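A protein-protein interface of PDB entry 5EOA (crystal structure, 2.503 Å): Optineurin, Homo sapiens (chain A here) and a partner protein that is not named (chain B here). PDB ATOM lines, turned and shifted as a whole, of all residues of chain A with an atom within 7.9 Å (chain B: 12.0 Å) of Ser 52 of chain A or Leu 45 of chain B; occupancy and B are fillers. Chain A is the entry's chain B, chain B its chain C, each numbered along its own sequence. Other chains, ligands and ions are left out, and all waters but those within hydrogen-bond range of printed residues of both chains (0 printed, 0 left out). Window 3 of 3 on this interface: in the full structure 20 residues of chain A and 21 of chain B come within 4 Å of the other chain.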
ATOM      1  N   LYS A  45      -1.340 -28.847  -0.422  1.00  0.00           N
ATOM      2  CA  LYS A  45      -2.374 -27.868  -0.745  1.00  0.00           C
ATOM      3  C   LYS A  45      -3.725 -28.307  -0.157  1.00  0.00           C
ATOM      4  O   LYS A  45      -4.395 -27.531   0.539  1.00  0.00           O
ATOM      5  CB  LYS A  45      -2.492 -27.726  -2.261  1.00  0.00           C
ATOM      6  CG  LYS A  45      -2.701 -26.313  -2.796  1.00  0.00           C
ATOM      7  CD  LYS A  45      -1.430 -25.790  -3.478  1.00  0.00           C
ATOM      8  CE  LYS A  45      -0.929 -26.744  -4.566  1.00  0.00           C
ATOM      9  NZ  LYS A  45       0.524 -26.561  -4.869  1.00  0.00           N
ATOM     10  N   GLY A  46      -4.097 -29.561  -0.417  1.00  0.00           N
ATOM     11  CA  GLY A  46      -5.380 -30.101  -0.008  1.00  0.00           C
ATOM     12  C   GLY A  46      -5.544 -30.106   1.499  1.00  0.00           C
ATOM     13  O   GLY A  46      -6.577 -29.679   2.006  1.00  0.00           O
ATOM     14  N   ARG A  47      -4.526 -30.582   2.212  1.00  0.00           N
ATOM     15  CA  ARG A  47      -4.532 -30.511   3.660  1.00  0.00           C
ATOM     16  C   ARG A  47      -4.630 -29.069   4.146  1.00  0.00           C
ATOM     17  O   ARG A  47      -5.395 -28.776   5.068  1.00  0.00           O
ATOM     18  CB  ARG A  47      -3.298 -31.175   4.242  1.00  0.00           C
ATOM     19  CG  ARG A  47      -3.256 -32.661   3.997  1.00  0.00           C
ATOM     20  CD  ARG A  47      -4.596 -33.309   4.246  1.00  0.00           C
ATOM     21  NE  ARG A  47      -4.494 -34.769   4.200  1.00  0.00           N
ATOM     22  CZ  ARG A  47      -5.494 -35.580   3.875  1.00  0.00           C
ATOM     23  NH1 ARG A  47      -6.686 -35.079   3.558  1.00  0.00           N
ATOM     24  NH2 ARG A  47      -5.304 -36.892   3.872  1.00  0.00           N
ATOM     25  N   PHE A  48      -3.863 -28.178   3.521  1.00  0.00           N
ATOM     26  CA  PHE A  48      -3.877 -26.775   3.907  1.00  0.00           C
ATOM     27  C   PHE A  48      -5.295 -26.211   3.832  1.00  0.00           C
ATOM     28  O   PHE A  48      -5.784 -25.605   4.784  1.00  0.00           O
ATOM     29  CB  PHE A  48      -2.940 -25.921   3.050  1.00  0.00           C
ATOM     30  CG  PHE A  48      -2.961 -24.480   3.438  1.00  0.00           C
ATOM     31  CD1 PHE A  48      -2.267 -24.042   4.565  1.00  0.00           C
ATOM     32  CD2 PHE A  48      -3.717 -23.562   2.726  1.00  0.00           C
ATOM     33  CE1 PHE A  48      -2.306 -22.700   4.955  1.00  0.00           C
ATOM     34  CE2 PHE A  48      -3.760 -22.226   3.121  1.00  0.00           C
ATOM     35  CZ  PHE A  48      -3.051 -21.802   4.233  1.00  0.00           C
ATOM     36  N   GLU A  49      -5.950 -26.416   2.700  1.00  0.00           N
ATOM     37  CA  GLU A  49      -7.310 -25.945   2.542  1.00  0.00           C
ATOM     38  C   GLU A  49      -8.259 -26.599   3.557  1.00  0.00           C
ATOM     39  O   GLU A  49      -9.114 -25.918   4.132  1.00  0.00           O
ATOM     40  CB  GLU A  49      -7.769 -26.151   1.100  1.00  0.00           C
ATOM     41  CG  GLU A  49      -7.046 -25.219   0.128  1.00  0.00           C
ATOM     42  CD  GLU A  49      -7.186 -25.637  -1.327  1.00  0.00           C
ATOM     43  OE1 GLU A  49      -7.659 -26.773  -1.595  1.00  0.00           O
ATOM     44  OE2 GLU A  49      -6.816 -24.822  -2.203  1.00  0.00           O
ATOM     45  N   GLU A  50      -8.084 -27.899   3.797  1.00  0.00           N
ATOM     46  CA  GLU A  50      -8.890 -28.609   4.790  1.00  0.00           C
ATOM     47  C   GLU A  50      -8.751 -28.022   6.199  1.00  0.00           C
ATOM     48  O   GLU A  50      -9.750 -27.745   6.860  1.00  0.00           O
ATOM     49  CB  GLU A  50      -8.559 -30.099   4.790  1.00  0.00           C
ATOM     50  CG  GLU A  50      -9.071 -30.829   3.556  1.00  0.00           C
ATOM     51  CD  GLU A  50      -8.533 -32.243   3.445  1.00  0.00           C
ATOM     52  OE1 GLU A  50      -7.777 -32.673   4.347  1.00  0.00           O
ATOM     53  OE2 GLU A  50      -8.861 -32.925   2.451  1.00  0.00           O
ATOM     54  N   LEU A  51      -7.513 -27.825   6.640  1.00  0.00           N
ATOM     55  CA  LEU A  51      -7.217 -27.258   7.948  1.00  0.00           C
ATOM     56  C   LEU A  51      -7.680 -25.809   8.061  1.00  0.00           C
ATOM     57  O   LEU A  51      -8.155 -25.362   9.116  1.00  0.00           O
ATOM     58  CB  LEU A  51      -5.716 -27.274   8.188  1.00  0.00           C
ATOM     59  CG  LEU A  51      -5.082 -28.630   8.385  1.00  0.00           C
ATOM     60  CD1 LEU A  51      -3.583 -28.436   8.400  1.00  0.00           C
ATOM     61  CD2 LEU A  51      -5.566 -29.235   9.687  1.00  0.00           C
ATOM     62  N   SER A  52      -7.505 -25.072   6.971  1.00  0.00           N
ATOM     63  CA  SER A  52      -7.951 -23.699   6.899  1.00  0.00           C
ATOM     64  C   SER A  52      -9.460 -23.640   7.208  1.00  0.00           C
ATOM     65  O   SER A  52      -9.879 -22.959   8.143  1.00  0.00           O
ATOM     66  CB  SER A  52      -7.633 -23.137   5.518  1.00  0.00           C
ATOM     67  OG  SER A  52      -8.013 -21.780   5.434  1.00  0.00           O
ATOM     68  N   ALA A  53     -10.249 -24.388   6.442  1.00  0.00           N
ATOM     69  CA  ALA A  53     -11.688 -24.471   6.624  1.00  0.00           C
ATOM     70  C   ALA A  53     -12.071 -24.887   8.046  1.00  0.00           C
ATOM     71  O   ALA A  53     -12.980 -24.321   8.657  1.00  0.00           O
ATOM     72  CB  ALA A  53     -12.275 -25.438   5.625  1.00  0.00           C
ATOM     73  N   TRP A  54     -11.350 -25.876   8.556  1.00  0.00           N
ATOM     74  CA  TRP A  54     -11.636 -26.518   9.830  1.00  0.00           C
ATOM     75  C   TRP A  54     -11.337 -25.603  11.020  1.00  0.00           C
ATOM     76  O   TRP A  54     -12.117 -25.522  11.970  1.00  0.00           O
ATOM     77  CB  TRP A  54     -10.813 -27.800   9.888  1.00  0.00           C
ATOM     78  CG  TRP A  54     -10.815 -28.560  11.162  1.00  0.00           C
ATOM     79  CD1 TRP A  54     -11.789 -29.400  11.624  1.00  0.00           C
ATOM     80  CD2 TRP A  54      -9.746 -28.627  12.111  1.00  0.00           C
ATOM     81  NE1 TRP A  54     -11.401 -29.957  12.822  1.00  0.00           N
ATOM     82  CE2 TRP A  54     -10.149 -29.498  13.139  1.00  0.00           C
ATOM     83  CE3 TRP A  54      -8.488 -28.024  12.196  1.00  0.00           C
ATOM     84  CZ2 TRP A  54      -9.337 -29.778  14.238  1.00  0.00           C
ATOM     85  CZ3 TRP A  54      -7.686 -28.304  13.282  1.00  0.00           C
ATOM     86  CH2 TRP A  54      -8.110 -29.177  14.288  1.00  0.00           C
ATOM     87  N   THR A  55     -10.204 -24.918  10.967  1.00  0.00           N
ATOM     88  CA  THR A  55      -9.871 -23.948  11.997  1.00  0.00           C
ATOM     89  C   THR A  55     -10.889 -22.800  12.011  1.00  0.00           C
ATOM     90  O   THR A  55     -11.294 -22.326  13.071  1.00  0.00           O
ATOM     91  CB  THR A  55      -8.457 -23.398  11.774  1.00  0.00           C
ATOM     92  OG1 THR A  55      -8.365 -22.850  10.452  1.00  0.00           O
ATOM     93  CG2 THR A  55      -7.421 -24.519  11.935  1.00  0.00           C
ATOM     94  N   GLU A  56     -11.298 -22.367  10.822  1.00  0.00           N
ATOM     95  CA  GLU A  56     -12.245 -21.279  10.674  1.00  0.00           C
ATOM     96  C   GLU A  56     -13.572 -21.686  11.317  1.00  0.00           C
ATOM     97  O   GLU A  56     -14.148 -20.937  12.118  1.00  0.00           O
ATOM     98  CB  GLU A  56     -12.416 -20.918   9.193  1.00  0.00           C
ATOM     99  CG  GLU A  56     -13.047 -19.558   8.939  1.00  0.00           C
ATOM    100  CD  GLU A  56     -12.369 -18.437   9.720  1.00  0.00           C
ATOM    101  OE1 GLU A  56     -11.118 -18.437   9.816  1.00  0.00           O
ATOM    102  OE2 GLU A  56     -13.090 -17.557  10.247  1.00  0.00           O
ATOM    103  N   LYS A  57     -14.024 -22.896  10.998  1.00  0.00           N
ATOM    104  CA  LYS A  57     -15.210 -23.440  11.624  1.00  0.00           C
ATOM    105  C   LYS A  57     -15.067 -23.415  13.148  1.00  0.00           C
ATOM    106  O   LYS A  57     -15.966 -22.924  13.825  1.00  0.00           O
ATOM    107  CB  LYS A  57     -15.525 -24.849  11.114  1.00  0.00           C
ATOM    108  CG  LYS A  57     -17.012 -25.197  11.194  1.00  0.00           C
ATOM    109  CD  LYS A  57     -17.324 -26.644  10.792  1.00  0.00           C
ATOM    110  CE  LYS A  57     -17.468 -27.564  12.001  1.00  0.00           C
ATOM    111  NZ  LYS A  57     -16.325 -27.441  12.965  1.00  0.00           N
ATOM    112  N   GLN A  58     -13.942 -23.906  13.677  1.00  0.00           N
ATOM    113  CA  GLN A  58     -13.699 -23.861  15.126  1.00  0.00           C
ATOM    114  C   GLN A  58     -13.846 -22.446  15.700  1.00  0.00           C
ATOM    115  O   GLN A  58     -14.435 -22.266  16.774  1.00  0.00           O
ATOM    116  CB  GLN A  58     -12.323 -24.405  15.476  1.00  0.00           C
ATOM    117  CG  GLN A  58     -12.325 -25.650  16.353  1.00  0.00           C
ATOM    118  CD  GLN A  58     -12.679 -26.892  15.585  1.00  0.00           C
ATOM    119  OE1 GLN A  58     -12.265 -27.057  14.442  1.00  0.00           O
ATOM    120  NE2 GLN A  58     -13.459 -27.772  16.200  1.00  0.00           N
ATOM    121  N   LYS A  59     -13.325 -21.445  14.991  1.00  0.00           N
ATOM    122  CA  LYS A  59     -13.406 -20.065  15.470  1.00  0.00           C
ATOM    123  C   LYS A  59     -14.854 -19.556  15.514  1.00  0.00           C
ATOM    124  O   LYS A  59     -15.297 -19.057  16.541  1.00  0.00           O
ATOM    125  CB  LYS A  59     -12.519 -19.146  14.631  1.00  0.00           C
ATOM    126  CG  LYS A  59     -11.032 -19.490  14.742  1.00  0.00           C
ATOM    127  CD  LYS A  59     -10.163 -18.668  13.788  1.00  0.00           C
ATOM    128  CE  LYS A  59      -8.696 -19.053  13.924  1.00  0.00           C
ATOM    129  NZ  LYS A  59      -7.797 -18.181  13.118  1.00  0.00           N
ATOM    130  N   ASN B  35       6.441 -26.901  -1.520  1.00  0.00           N
ATOM    131  CA  ASN B  35       6.282 -27.532  -0.219  1.00  0.00           C
ATOM    132  C   ASN B  35       6.655 -26.594   0.939  1.00  0.00           C
ATOM    133  O   ASN B  35       5.873 -26.399   1.860  1.00  0.00           O
ATOM    134  CB  ASN B  35       7.143 -28.796  -0.178  1.00  0.00           C
ATOM    135  CG  ASN B  35       6.609 -29.835   0.768  1.00  0.00           C
ATOM    136  OD1 ASN B  35       7.129 -30.017   1.875  1.00  0.00           O
ATOM    137  ND2 ASN B  35       5.572 -30.545   0.333  1.00  0.00           N
ATOM    138  N   ASN B  36       7.842 -25.999   0.876  1.00  0.00           N
ATOM    139  CA  ASN B  36       8.268 -25.032   1.884  1.00  0.00           C
ATOM    140  C   ASN B  36       7.305 -23.843   1.989  1.00  0.00           C
ATOM    141  O   ASN B  36       7.043 -23.339   3.070  1.00  0.00           O
ATOM    142  CB  ASN B  36       9.680 -24.499   1.590  1.00  0.00           C
ATOM    143  CG  ASN B  36      10.770 -25.546   1.787  1.00  0.00           C
ATOM    144  OD1 ASN B  36      10.656 -26.441   2.624  1.00  0.00           O
ATOM    145  ND2 ASN B  36      11.848 -25.420   1.018  1.00  0.00           N
ATOM    146  N   HIS B  37       6.814 -23.374   0.851  1.00  0.00           N
ATOM    147  CA  HIS B  37       5.949 -22.214   0.845  1.00  0.00           C
ATOM    148  C   HIS B  37       4.690 -22.483   1.668  1.00  0.00           C
ATOM    149  O   HIS B  37       4.294 -21.677   2.511  1.00  0.00           O
ATOM    150  CB  HIS B  37       5.558 -21.866  -0.587  1.00  0.00           C
ATOM    151  CG  HIS B  37       4.432 -20.884  -0.674  1.00  0.00           C
ATOM    152  ND1 HIS B  37       4.446 -19.672  -0.014  1.00  0.00           N
ATOM    153  CD2 HIS B  37       3.254 -20.937  -1.341  1.00  0.00           C
ATOM    154  CE1 HIS B  37       3.333 -19.017  -0.284  1.00  0.00           C
ATOM    155  NE2 HIS B  37       2.593 -19.761  -1.087  1.00  0.00           N
ATOM    156  N   ILE B  38       4.083 -23.637   1.413  1.00  0.00           N
ATOM    157  CA  ILE B  38       2.861 -24.052   2.067  1.00  0.00           C
ATOM    158  C   ILE B  38       3.110 -24.326   3.550  1.00  0.00           C
ATOM    159  O   ILE B  38       2.340 -23.893   4.401  1.00  0.00           O
ATOM    160  CB  ILE B  38       2.279 -25.280   1.348  1.00  0.00           C
ATOM    161  CG1 ILE B  38       1.934 -24.902  -0.089  1.00  0.00           C
ATOM    162  CG2 ILE B  38       1.050 -25.806   2.049  1.00  0.00           C
ATOM    163  CD1 ILE B  38       1.766 -26.078  -0.998  1.00  0.00           C
ATOM    164  N   LEU B  39       4.196 -25.030   3.854  1.00  0.00           N
ATOM    165  CA  LEU B  39       4.581 -25.291   5.241  1.00  0.00           C
ATOM    166  C   LEU B  39       4.631 -24.011   6.070  1.00  0.00           C
ATOM    167  O   LEU B  39       4.200 -23.999   7.219  1.00  0.00           O
ATOM    168  CB  LEU B  39       5.940 -25.994   5.297  1.00  0.00           C
ATOM    169  CG  LEU B  39       6.528 -26.177   6.698  1.00  0.00           C
ATOM    170  CD1 LEU B  39       5.530 -26.870   7.623  1.00  0.00           C
ATOM    171  CD2 LEU B  39       7.805 -26.983   6.629  1.00  0.00           C
ATOM    172  N   GLU B  40       5.163 -22.944   5.484  1.00  0.00           N
ATOM    173  CA  GLU B  40       5.238 -21.648   6.146  1.00  0.00           C
ATOM    174  C   GLU B  40       3.838 -21.141   6.489  1.00  0.00           C
ATOM    175  O   GLU B  40       3.600 -20.605   7.564  1.00  0.00           O
ATOM    176  CB  GLU B  40       5.932 -20.648   5.225  1.00  0.00           C
ATOM    177  CG  GLU B  40       7.207 -20.066   5.789  1.00  0.00           C
ATOM    178  CD  GLU B  40       6.943 -19.019   6.842  1.00  0.00           C
ATOM    179  OE1 GLU B  40       6.265 -18.014   6.527  1.00  0.00           O
ATOM    180  OE2 GLU B  40       7.413 -19.202   7.985  1.00  0.00           O
ATOM    181  N   ARG B  41       2.920 -21.326   5.546  1.00  0.00           N
ATOM    182  CA  ARG B  41       1.541 -20.924   5.700  1.00  0.00           C
ATOM    183  C   ARG B  41       0.794 -21.677   6.808  1.00  0.00           C
ATOM    184  O   ARG B  41      -0.099 -21.105   7.434  1.00  0.00           O
ATOM    185  CB  ARG B  41       0.812 -21.053   4.368  1.00  0.00           C
ATOM    186  CG  ARG B  41       1.314 -20.081   3.334  1.00  0.00           C
ATOM    187  CD  ARG B  41       0.895 -18.663   3.657  1.00  0.00           C
ATOM    188  NE  ARG B  41       1.289 -17.748   2.595  1.00  0.00           N
ATOM    189  CZ  ARG B  41       0.490 -17.380   1.598  1.00  0.00           C
ATOM    190  NH1 ARG B  41      -0.755 -17.834   1.535  1.00  0.00           N
ATOM    191  NH2 ARG B  41       0.931 -16.546   0.669  1.00  0.00           N
ATOM    192  N   PHE B  42       1.156 -22.939   7.054  1.00  0.00           N
ATOM    193  CA  PHE B  42       0.553 -23.717   8.141  1.00  0.00           C
ATOM    194  C   PHE B  42       0.699 -22.967   9.453  1.00  0.00           C
ATOM    195  O   PHE B  42      -0.244 -22.889  10.247  1.00  0.00           O
ATOM    196  CB  PHE B  42       1.242 -25.066   8.310  1.00  0.00           C
ATOM    197  CG  PHE B  42       0.690 -26.168   7.441  1.00  0.00           C
ATOM    198  CD1 PHE B  42       0.745 -26.088   6.064  1.00  0.00           C
ATOM    199  CD2 PHE B  42       0.179 -27.322   8.010  1.00  0.00           C
ATOM    200  CE1 PHE B  42       0.257 -27.122   5.269  1.00  0.00           C
ATOM    201  CE2 PHE B  42      -0.302 -28.359   7.217  1.00  0.00           C
ATOM    202  CZ  PHE B  42      -0.256 -28.255   5.846  1.00  0.00           C
ATOM    203  N   GLY B  43       1.888 -22.405   9.663  1.00  0.00           N
ATOM    204  CA  GLY B  43       2.205 -21.715  10.898  1.00  0.00           C
ATOM    205  C   GLY B  43       1.243 -20.602  11.265  1.00  0.00           C
ATOM    206  O   GLY B  43       1.195 -20.192  12.421  1.00  0.00           O
ATOM    207  N   SER B  44       0.465 -20.133  10.292  1.00  0.00           N
ATOM    208  CA  SER B  44      -0.421 -18.987  10.488  1.00  0.00           C
ATOM    209  C   SER B  44      -1.888 -19.363  10.631  1.00  0.00           C
ATOM    210  O   SER B  44      -2.736 -18.479  10.686  1.00  0.00           O
ATOM    211  CB  SER B  44      -0.296 -18.028   9.308  1.00  0.00           C
ATOM    212  OG  SER B  44      -0.979 -18.541   8.172  1.00  0.00           O
ATOM    213  N   LEU B  45      -2.195 -20.658  10.671  1.00  0.00           N
ATOM    214  CA  LEU B  45      -3.592 -21.093  10.732  1.00  0.00           C
ATOM    215  C   LEU B  45      -4.244 -20.813  12.082  1.00  0.00           C
ATOM    216  O   LEU B  45      -5.407 -20.424  12.134  1.00  0.00           O
ATOM    217  CB  LEU B  45      -3.720 -22.573  10.388  1.00  0.00           C
ATOM    218  CG  LEU B  45      -3.589 -22.935   8.912  1.00  0.00           C
ATOM    219  CD1 LEU B  45      -3.422 -24.428   8.755  1.00  0.00           C
ATOM    220  CD2 LEU B  45      -4.809 -22.471   8.169  1.00  0.00           C
ATOM    221  N   THR B  46      -3.500 -21.023  13.166  1.00  0.00           N
ATOM    222  CA  THR B  46      -4.003 -20.724  14.507  1.00  0.00           C
ATOM    223  C   THR B  46      -4.021 -19.213  14.766  1.00  0.00           C
ATOM    224  O   THR B  46      -4.952 -18.695  15.379  1.00  0.00           O
ATOM    225  CB  THR B  46      -3.167 -21.417  15.601  1.00  0.00           C
ATOM    226  OG1 THR B  46      -1.823 -20.925  15.560  1.00  0.00           O
ATOM    227  CG2 THR B  46      -3.146 -22.924  15.395  1.00  0.00           C
ATOM    228  N   MET B  47      -2.993 -18.512  14.291  1.00  0.00           N
ATOM    229  CA  MET B  47      -2.896 -17.065  14.474  1.00  0.00           C
ATOM    230  C   MET B  47      -4.055 -16.337  13.795  1.00  0.00           C
ATOM    231  O   MET B  47      -4.480 -16.717  12.701  1.00  0.00           O
ATOM    232  CB  MET B  47      -1.562 -16.539  13.931  1.00  0.00           C
ATOM    233  CG  MET B  47      -0.330 -17.162  14.577  1.00  0.00           C
ATOM    234  SD  MET B  47      -0.147 -16.792  16.341  1.00  0.00           S
ATOM    235  CE  MET B  47       0.302 -18.424  16.980  1.00  0.00           C
ATOM    236  N   ASP B  48      -4.566 -15.295  14.450  1.00  0.00           N
ATOM    237  CA  ASP B  48      -5.689 -14.529  13.914  1.00  0.00           C
ATOM    238  C   ASP B  48      -5.294 -13.116  13.487  1.00  0.00           C
ATOM    239  O   ASP B  48      -5.050 -12.857  12.304  1.00  0.00           O
ATOM    240  CB  ASP B  48      -6.834 -14.477  14.929  1.00  0.00           C
ATOM    241  CG  ASP B  48      -6.342 -14.334  16.354  1.00  0.00           C
ATOM    242  OD1 ASP B  48      -5.915 -15.357  16.937  1.00  0.00           O
ATOM    243  OD2 ASP B  48      -6.385 -13.206  16.890  1.00  0.00           O
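The backbone carbonyl oxygen of Leu 45 of chain B sits at hydrogen-bond distance from the side-chain amino group of Lys 59 of chain A (3.4 Å).
O of Leu 51 of chain A sits at hydrogen-bond distance from OG1 of Thr 55 of chain A (2.9 Å).
OG1 of Thr 55 of chain A is in hydrogen-bond range of O of Ser 52 of chain A.
The side-chain hydroxyl (OG) of Ser 44 of chain B lies within hydrogen-bond range of the backbone carbonyl oxygen (O) of Arg 41 of chain B (2.8 Å).
Among the printed residues, pairs that only touch across the chains: Phe 48 of chain A with Arg 41 of chain B, Phe 48 of chain A with Phe 42 of chain B, Leu 51 of chain A with Phe 42 of chain B, Leu 51 of chain A with Leu 45 of chain B, Ser 52 of chain A with Leu 45 of chain B, Lys 59 of chain A with Thr 46 of chain B and Lys 59 of chain A with Met 47 of chain B.
Ser 52 of chain A touches just one residue of chain B: Leu 45 (3.6 Å).
Phe 48 of chain A touches just these residues of chain B: Arg 41 and Phe 42.
Leu 51 of chain A touches just these residues of chain B: Phe 42 and Leu 45.
Ala 53 of chain A touches none of the printed residues of chain B.
No residue of chain B comes within 4 Å of Thr 55 of chain A.
No residue of chain B comes within 4 Å of Glu 56 of chain A.
No residue of chain A comes within 4 Å of Ser 44 of chain B.
Printed residues of chain A within 4 Å of Thr 46 of chain B: Lys 59.
Of the printed residues of chain B, Lys 59 of chain A touches Leu 45 (3.4 Å), Thr 46 (3.7 Å) and Met 47 (3.6 Å).
Of the printed residues of chain A, Phe 42 of chain B touches Phe 48 and Leu 51.
The nearest residue of chain B that does not touch Ser 52 of chain A is Phe 42 of chain B (7.9 Å).
The nearest printed residue of chain A that does not touch Phe 42 of chain B is Arg 47 of chain A (4.5 Å).
Of the 15 printed residues of chain A, 4 touch a printed residue of chain B.
Hydrophobic or aromatic side chains of chain A within 4 Å of the printed part of chain B: Phe 48 and Leu 51.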
